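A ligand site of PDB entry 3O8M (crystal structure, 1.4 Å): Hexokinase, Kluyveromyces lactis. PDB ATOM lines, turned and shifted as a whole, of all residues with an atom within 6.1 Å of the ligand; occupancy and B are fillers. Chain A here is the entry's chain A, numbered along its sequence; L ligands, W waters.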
ATOM      1  N   GLY A  88     -33.724 -17.791  -9.073  1.00  0.00           N
ATOM      2  CA  GLY A  88     -33.142 -16.435  -9.259  1.00  0.00           C
ATOM      3  C   GLY A  88     -34.142 -15.345  -9.675  1.00  0.00           C
ATOM      4  O   GLY A  88     -33.768 -14.150  -9.752  1.00  0.00           O
ATOM      5  N   PHE A 156     -29.787 -22.573 -12.084  1.00  0.00           N
ATOM      6  CA  PHE A 156     -29.138 -21.957 -10.867  1.00  0.00           C
ATOM      7  C   PHE A 156     -28.489 -20.675 -11.389  1.00  0.00           C
ATOM      8  O   PHE A 156     -27.454 -20.751 -12.015  1.00  0.00           O
ATOM      9  CB  PHE A 156     -28.148 -23.001 -10.253  1.00  0.00           C
ATOM     10  CG  PHE A 156     -27.458 -22.544  -9.022  1.00  0.00           C
ATOM     11  CD1 PHE A 156     -28.183 -22.404  -7.871  1.00  0.00           C
ATOM     12  CD2 PHE A 156     -26.074 -22.357  -9.002  1.00  0.00           C
ATOM     13  CE1 PHE A 156     -27.518 -21.956  -6.672  1.00  0.00           C
ATOM     14  CE2 PHE A 156     -25.410 -21.938  -7.813  1.00  0.00           C
ATOM     15  CZ  PHE A 156     -26.177 -21.774  -6.673  1.00  0.00           C
ATOM     16  N   SER A 157     -29.126 -19.531 -11.091  1.00  0.00           N
ATOM     17  CA  SER A 157     -28.718 -18.254 -11.706  1.00  0.00           C
ATOM     18  C   SER A 157     -27.539 -17.565 -10.996  1.00  0.00           C
ATOM     19  O   SER A 157     -27.636 -16.385 -10.705  1.00  0.00           O
ATOM     20  CB  SER A 157     -29.916 -17.299 -11.800  1.00  0.00           C
ATOM     21  OG  SER A 157     -30.999 -18.004 -12.391  1.00  0.00           O
ATOM     22  N   TYR A 158     -26.478 -18.325 -10.727  1.00  0.00           N
ATOM     23  CA  TYR A 158     -25.266 -17.925  -9.995  1.00  0.00           C
ATOM     24  C   TYR A 158     -24.106 -18.671 -10.619  1.00  0.00           C
ATOM     25  O   TYR A 158     -24.314 -19.682 -11.213  1.00  0.00           O
ATOM     26  CB  TYR A 158     -25.419 -18.259  -8.432  1.00  0.00           C
ATOM     27  CG  TYR A 158     -26.713 -17.635  -7.891  1.00  0.00           C
ATOM     28  CD1 TYR A 158     -26.771 -16.241  -7.500  1.00  0.00           C
ATOM     29  CD2 TYR A 158     -27.911 -18.356  -7.877  1.00  0.00           C
ATOM     30  CE1 TYR A 158     -27.987 -15.641  -7.117  1.00  0.00           C
ATOM     31  CE2 TYR A 158     -29.134 -17.747  -7.547  1.00  0.00           C
ATOM     32  CZ  TYR A 158     -29.145 -16.389  -7.171  1.00  0.00           C
ATOM     33  OH  TYR A 158     -30.484 -15.985  -6.886  1.00  0.00           O
ATOM     34  N   PRO A 159     -22.888 -18.177 -10.443  1.00  0.00           N
ATOM     35  CA  PRO A 159     -21.742 -18.808 -11.119  1.00  0.00           C
ATOM     36  C   PRO A 159     -21.367 -20.155 -10.473  1.00  0.00           C
ATOM     37  O   PRO A 159     -21.202 -20.224  -9.244  1.00  0.00           O
ATOM     38  CB  PRO A 159     -20.576 -17.773 -10.927  1.00  0.00           C
ATOM     39  CG  PRO A 159     -20.979 -16.982  -9.663  1.00  0.00           C
ATOM     40  CD  PRO A 159     -22.553 -16.890  -9.766  1.00  0.00           C
ATOM     41  N   ARG A 172     -19.312 -17.830  -6.220  1.00  0.00           N
ATOM     42  CA  ARG A 172     -19.458 -16.658  -5.350  1.00  0.00           C
ATOM     43  C   ARG A 172     -20.970 -16.373  -5.435  1.00  0.00           C
ATOM     44  O   ARG A 172     -21.567 -16.527  -6.474  1.00  0.00           O
ATOM     45  CB  ARG A 172     -18.695 -15.436  -5.934  1.00  0.00           C
ATOM     46  CG  ARG A 172     -19.106 -15.074  -7.398  1.00  0.00           C
ATOM     47  CD  ARG A 172     -18.101 -14.051  -8.090  1.00  0.00           C
ATOM     48  NE  ARG A 172     -16.782 -14.695  -8.187  1.00  0.00           N
ATOM     49  CZ  ARG A 172     -16.534 -15.742  -9.013  1.00  0.00           C
ATOM     50  NH1 ARG A 172     -17.414 -16.080  -9.968  1.00  0.00           N
ATOM     51  NH2 ARG A 172     -15.379 -16.340  -8.880  1.00  0.00           N
ATOM     52  N   THR A 174     -23.854 -13.689  -5.804  1.00  0.00           N
ATOM     53  CA  THR A 174     -23.996 -12.403  -6.476  1.00  0.00           C
ATOM     54  C   THR A 174     -25.386 -11.851  -6.154  1.00  0.00           C
ATOM     55  O   THR A 174     -26.256 -12.512  -5.500  1.00  0.00           O
ATOM     56  CB  THR A 174     -23.779 -12.612  -8.005  1.00  0.00           C
ATOM     57  OG1 THR A 174     -24.804 -13.484  -8.510  1.00  0.00           O
ATOM     58  CG2 THR A 174     -22.377 -13.143  -8.288  1.00  0.00           C
ATOM     59  N   LYS A 175     -25.595 -10.599  -6.605  1.00  0.00           N
ATOM     60  CA  LYS A 175     -26.957  -9.981  -6.519  1.00  0.00           C
ATOM     61  C   LYS A 175     -27.458  -9.870  -5.069  1.00  0.00           C
ATOM     62  O   LYS A 175     -28.600 -10.213  -4.763  1.00  0.00           O
ATOM     63  CB  LYS A 175     -27.992 -10.714  -7.423  1.00  0.00           C
ATOM     64  CG  LYS A 175     -27.556 -10.638  -8.921  1.00  0.00           C
ATOM     65  CD  LYS A 175     -28.449 -11.564  -9.729  1.00  0.00           C
ATOM     66  CE  LYS A 175     -28.181 -13.059  -9.546  1.00  0.00           C
ATOM     67  NZ  LYS A 175     -28.880 -13.853 -10.626  1.00  0.00           N
ATOM     68  N   ASN A 209     -26.883 -22.433 -16.130  1.00  0.00           N
ATOM     69  CA  ASN A 209     -27.096 -21.026 -15.836  1.00  0.00           C
ATOM     70  C   ASN A 209     -28.241 -20.457 -16.640  1.00  0.00           C
ATOM     71  O   ASN A 209     -28.586 -20.990 -17.719  1.00  0.00           O
ATOM     72  CB  ASN A 209     -25.769 -20.257 -16.188  1.00  0.00           C
ATOM     73  CG  ASN A 209     -25.781 -18.836 -15.652  1.00  0.00           C
ATOM     74  OD1 ASN A 209     -25.943 -17.881 -16.466  1.00  0.00           O
ATOM     75  ND2 ASN A 209     -25.693 -18.652 -14.386  1.00  0.00           N
ATOM     76  N   ASP A 210     -28.816 -19.364 -16.147  1.00  0.00           N
ATOM     77  CA  ASP A 210     -29.917 -18.693 -16.874  1.00  0.00           C
ATOM     78  C   ASP A 210     -29.517 -18.150 -18.260  1.00  0.00           C
ATOM     79  O   ASP A 210     -30.339 -18.155 -19.163  1.00  0.00           O
ATOM     80  CB  ASP A 210     -30.667 -17.700 -15.993  1.00  0.00           C
ATOM     81  CG  ASP A 210     -29.759 -16.687 -15.322  1.00  0.00           C
ATOM     82  OD1 ASP A 210     -28.596 -16.986 -15.017  1.00  0.00           O
ATOM     83  OD2 ASP A 210     -30.318 -15.531 -15.058  1.00  0.00           O
ATOM     84  N   THR A 211     -28.245 -17.755 -18.410  1.00  0.00           N
ATOM     85  CA  THR A 211     -27.806 -17.323 -19.758  1.00  0.00           C
ATOM     86  C   THR A 211     -27.749 -18.452 -20.728  1.00  0.00           C
ATOM     87  O   THR A 211     -28.246 -18.331 -21.862  1.00  0.00           O
ATOM     88  CB  THR A 211     -26.451 -16.579 -19.677  1.00  0.00           C
ATOM     89  OG1 THR A 211     -25.452 -17.451 -19.186  1.00  0.00           O
ATOM     90  CG2 THR A 211     -26.553 -15.299 -18.845  1.00  0.00           C
ATOM     91  N   ILE A 230     -28.834 -11.791 -20.122  1.00  0.00           N
ATOM     92  CA  ILE A 230     -29.760 -11.293 -19.096  1.00  0.00           C
ATOM     93  C   ILE A 230     -29.363  -9.909 -18.744  1.00  0.00           C
ATOM     94  O   ILE A 230     -28.186  -9.626 -18.471  1.00  0.00           O
ATOM     95  CB  ILE A 230     -29.717 -12.228 -17.848  1.00  0.00           C
ATOM     96  CG1 ILE A 230     -30.147 -13.677 -18.261  1.00  0.00           C
ATOM     97  CG2 ILE A 230     -30.656 -11.650 -16.736  1.00  0.00           C
ATOM     98  CD1 ILE A 230     -31.592 -13.812 -18.765  1.00  0.00           C
ATOM     99  N   GLY A 232     -31.049  -7.788 -16.042  1.00  0.00           N
ATOM    100  CA  GLY A 232     -32.099  -7.853 -15.060  1.00  0.00           C
ATOM    101  C   GLY A 232     -31.531  -7.639 -13.721  1.00  0.00           C
ATOM    102  O   GLY A 232     -30.765  -6.728 -13.518  1.00  0.00           O
ATOM    103  N   THR A 233     -31.889  -8.456 -12.743  1.00  0.00           N
ATOM    104  CA  THR A 233     -31.364  -8.289 -11.435  1.00  0.00           C
ATOM    105  C   THR A 233     -29.816  -8.360 -11.547  1.00  0.00           C
ATOM    106  O   THR A 233     -29.115  -7.582 -10.858  1.00  0.00           O
ATOM    107  CB  THR A 233     -31.860  -9.384 -10.534  1.00  0.00           C
ATOM    108  OG1 THR A 233     -33.300  -9.400 -10.561  1.00  0.00           O
ATOM    109  CG2 THR A 233     -31.509  -9.057  -9.040  1.00  0.00           C
ATOM    110  N   GLY A 234     -29.341  -9.252 -12.436  1.00  0.00           N
ATOM    111  CA  GLY A 234     -27.903  -9.264 -12.740  1.00  0.00           C
ATOM    112  C   GLY A 234     -27.696  -8.985 -14.194  1.00  0.00           C
ATOM    113  O   GLY A 234     -28.630  -8.931 -15.001  1.00  0.00           O
ATOM    114  N   VAL A 235     -26.413  -9.083 -14.592  1.00  0.00           N
ATOM    115  CA  VAL A 235     -26.045  -8.849 -16.021  1.00  0.00           C
ATOM    116  C   VAL A 235     -25.029  -9.921 -16.339  1.00  0.00           C
ATOM    117  O   VAL A 235     -23.969 -10.058 -15.693  1.00  0.00           O
ATOM    118  CB  VAL A 235     -25.412  -7.416 -16.181  1.00  0.00           C
ATOM    119  CG1 VAL A 235     -24.465  -7.336 -17.427  1.00  0.00           C
ATOM    120  CG2 VAL A 235     -26.581  -6.396 -16.350  1.00  0.00           C
ATOM    121  N   ASN A 236     -25.284 -10.664 -17.417  1.00  0.00           N
ATOM    122  CA  ASN A 236     -24.382 -11.725 -17.832  1.00  0.00           C
ATOM    123  C   ASN A 236     -24.760 -12.152 -19.273  1.00  0.00           C
ATOM    124  O   ASN A 236     -25.798 -11.725 -19.812  1.00  0.00           O
ATOM    125  CB  ASN A 236     -24.623 -12.940 -16.876  1.00  0.00           C
ATOM    126  CG  ASN A 236     -23.602 -14.075 -17.057  1.00  0.00           C
ATOM    127  OD1 ASN A 236     -22.550 -13.891 -17.698  1.00  0.00           O
ATOM    128  ND2 ASN A 236     -23.924 -15.252 -16.493  1.00  0.00           N
ATOM    129  N   GLY A 237     -23.955 -13.015 -19.889  1.00  0.00           N
ATOM    130  CA  GLY A 237     -24.211 -13.523 -21.237  1.00  0.00           C
ATOM    131  C   GLY A 237     -23.615 -14.900 -21.426  1.00  0.00           C
ATOM    132  O   GLY A 237     -22.576 -15.199 -20.878  1.00  0.00           O
ATOM    133  N   ASN A 266     -21.091 -20.065 -20.201  1.00  0.00           N
ATOM    134  CA  ASN A 266     -21.650 -19.082 -19.347  1.00  0.00           C
ATOM    135  C   ASN A 266     -20.488 -18.113 -18.979  1.00  0.00           C
ATOM    136  O   ASN A 266     -19.641 -18.450 -18.174  1.00  0.00           O
ATOM    137  CB  ASN A 266     -22.151 -19.811 -18.062  1.00  0.00           C
ATOM    138  CG  ASN A 266     -22.466 -18.780 -16.967  1.00  0.00           C
ATOM    139  OD1 ASN A 266     -22.636 -17.599 -17.312  1.00  0.00           O
ATOM    140  ND2 ASN A 266     -22.571 -19.199 -15.705  1.00  0.00           N
ATOM    141  N   GLU A 268     -20.207 -15.415 -17.248  1.00  0.00           N
ATOM    142  CA  GLU A 268     -20.225 -14.655 -15.936  1.00  0.00           C
ATOM    143  C   GLU A 268     -19.518 -13.321 -16.066  1.00  0.00           C
ATOM    144  O   GLU A 268     -18.753 -12.929 -15.198  1.00  0.00           O
ATOM    145  CB  GLU A 268     -19.568 -15.533 -14.805  1.00  0.00           C
ATOM    146  CG  GLU A 268     -20.438 -16.730 -14.403  1.00  0.00           C
ATOM    147  CD  GLU A 268     -21.708 -16.296 -13.699  1.00  0.00           C
ATOM    148  OE1 GLU A 268     -21.768 -15.153 -13.151  1.00  0.00           O
ATOM    149  OE2 GLU A 268     -22.664 -17.093 -13.670  1.00  0.00           O
ATOM    150  N   GLY A 270     -20.667 -10.453 -15.739  1.00  0.00           N
ATOM    151  CA  GLY A 270     -20.930  -9.499 -14.661  1.00  0.00           C
ATOM    152  C   GLY A 270     -19.658  -9.173 -13.858  1.00  0.00           C
ATOM    153  O   GLY A 270     -19.532  -8.111 -13.207  1.00  0.00           O
ATOM    154  N   GLN A 298     -17.913  -8.652  -9.182  1.00  0.00           N
ATOM    155  CA  GLN A 298     -19.053  -8.208 -10.043  1.00  0.00           C
ATOM    156  C   GLN A 298     -18.999  -6.720 -10.383  1.00  0.00           C
ATOM    157  O   GLN A 298     -20.039  -6.060 -10.456  1.00  0.00           O
ATOM    158  CB  GLN A 298     -20.399  -8.636  -9.425  1.00  0.00           C
ATOM    159  CG  GLN A 298     -20.479 -10.193  -9.206  1.00  0.00           C
ATOM    160  CD  GLN A 298     -20.383 -10.994 -10.493  1.00  0.00           C
ATOM    161  OE1 GLN A 298     -19.329 -11.583 -10.796  1.00  0.00           O
ATOM    162  NE2 GLN A 298     -21.510 -11.044 -11.280  1.00  0.00           N
ATOM    163  N   GLU A 301     -21.389  -5.685 -13.458  1.00  0.00           N
ATOM    164  CA  GLU A 301     -22.794  -5.824 -13.066  1.00  0.00           C
ATOM    165  C   GLU A 301     -23.224  -4.796 -12.045  1.00  0.00           C
ATOM    166  O   GLU A 301     -24.359  -4.252 -12.187  1.00  0.00           O
ATOM    167  CB  GLU A 301     -22.948  -7.238 -12.476  1.00  0.00           C
ATOM    168  CG  GLU A 301     -24.130  -7.479 -11.588  1.00  0.00           C
ATOM    169  CD  GLU A 301     -24.273  -8.929 -11.393  1.00  0.00           C
ATOM    170  OE1 GLU A 301     -23.834  -9.508 -10.375  1.00  0.00           O
ATOM    171  OE2 GLU A 301     -24.836  -9.572 -12.278  1.00  0.00           O
HETATM  172  C1  LIG L   1     -25.466 -12.667 -12.001  1.00  0.00           C
HETATM  173  C2  LIG L   1     -25.152 -14.148 -11.833  1.00  0.00           C
HETATM  174  C3  LIG L   1     -25.194 -14.879 -13.170  1.00  0.00           C
HETATM  175  C4  LIG L   1     -26.586 -14.714 -13.814  1.00  0.00           C
HETATM  176  C5  LIG L   1     -26.872 -13.228 -13.859  1.00  0.00           C
HETATM  177  C6  LIG L   1     -28.310 -12.913 -14.354  1.00  0.00           C
HETATM  178  O1  LIG L   1     -24.570 -12.047 -12.910  1.00  0.00           O
HETATM  179  O2  LIG L   1     -23.785 -14.256 -11.246  1.00  0.00           O
HETATM  180  O3  LIG L   1     -25.029 -16.327 -12.908  1.00  0.00           O
HETATM  181  O4  LIG L   1     -26.549 -15.250 -15.131  1.00  0.00           O
HETATM  182  O5  LIG L   1     -26.786 -12.640 -12.556  1.00  0.00           O
HETATM  183  O6  LIG L   1     -29.332 -13.612 -13.603  1.00  0.00           O
HETATM  184  O   HOH W   1     -21.982 -12.444 -14.058  1.00  0.00           O
HETATM  185  O   HOH W   2     -31.068 -11.557 -13.121  1.00  0.00           O
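An oxygen (O1) of the ligand is in hydrogen-bond range of the side-chain carboxylate (OE2) of Glu 301 (2.6 Å).
The side-chain carboxylate (OE2) of Glu 268 lies within hydrogen-bond range of an oxygen (O3) of the ligand (2.6 Å).
The side-chain carboxylate of Asp 210 sits at hydrogen-bond distance from an oxygen (O6) of the ligand, at 2.6 Å.
An oxygen (O3) of the ligand lies within hydrogen-bond range of the side-chain amide nitrogen (ND2) of Asn 209.
An oxygen (O4) of the ligand sits at hydrogen-bond distance from the side-chain amide nitrogen (ND2) of Asn 236, 3.0 Å away.
The side-chain hydroxyl (OG1) of Thr 174 sits at hydrogen-bond distance from an oxygen (O2) of the ligand (3.0 Å).
The side-chain amino group (NZ) of Lys 175 lies within hydrogen-bond range of an oxygen (O6) of the ligand, at 3.0 Å.
N of Tyr 158 is in hydrogen-bond range of O3 of the ligand, at 3.3 Å.
O of Ser 157 lies close to O3 of the ligand (3.4 Å).
The backbone carbonyl oxygen of Val 235 sits at hydrogen-bond distance from an oxygen (O1) of the ligand (3.5 Å).
N of Val 235 sits at hydrogen-bond distance from OE2 of Glu 301, at 2.8 Å.
The side-chain amide nitrogen of Gln 298 sits at hydrogen-bond distance from the side-chain carboxylate of Glu 301, 2.9 Å away.
OE2 of Glu 268 is in hydrogen-bond range of ND2 of Asn 266 (2.9 Å).
The side-chain carboxylate (OD1) of Asp 210 lies close to the side-chain amide oxygen (OD1) of Asn 209, at 3.2 Å.
The side-chain amide nitrogen (ND2) of Asn 236 is in hydrogen-bond range of the side-chain amide oxygen (OD1) of Asn 209, 3.3 Å away.
OD1 of Asn 266 lies within hydrogen-bond range of ND2 of Asn 236, at 2.8 Å.
The side-chain amino group (NZ) of Lys 175 is in hydrogen-bond range of the backbone carbonyl oxygen (O) of Ser 157 (2.8 Å).
O of Val 235 sits close to N of Gly 270, at 3.3 Å.
Residues that only touch the ligand: Pro 159 (3.3 Å), Thr 211 (3.7 Å), Ile 230 (3.6 Å), Gly 234 (3.6 Å) and Gln 298 (3.6 Å).
Hydrophobic or aromatic side chains within 4 Å of the ligand: Pro 159 and Ile 230.
Of the 23 residues printed, 15 come within 4 Å of the ligand.
Along chain A the residues within 4 Å of the ligand span positions 157 to 301.
The nearest printed residue that does not touch the ligand is Asn 266 (4.7 Å).
Water W2 lies within hydrogen-bond range of O6 of the ligand (2.7 Å), N of Gly 234 (3.0 Å) and N of Thr 233 (3.2 Å).
Water W1 lies within hydrogen-bond range of an oxygen (O1) of the ligand (2.9 Å), the side-chain carboxylate of Glu 268 (2.9 Å), the backbone NH of Gly 270 (2.9 Å) and the side-chain amide nitrogen of Gln 298 (3.1 Å).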
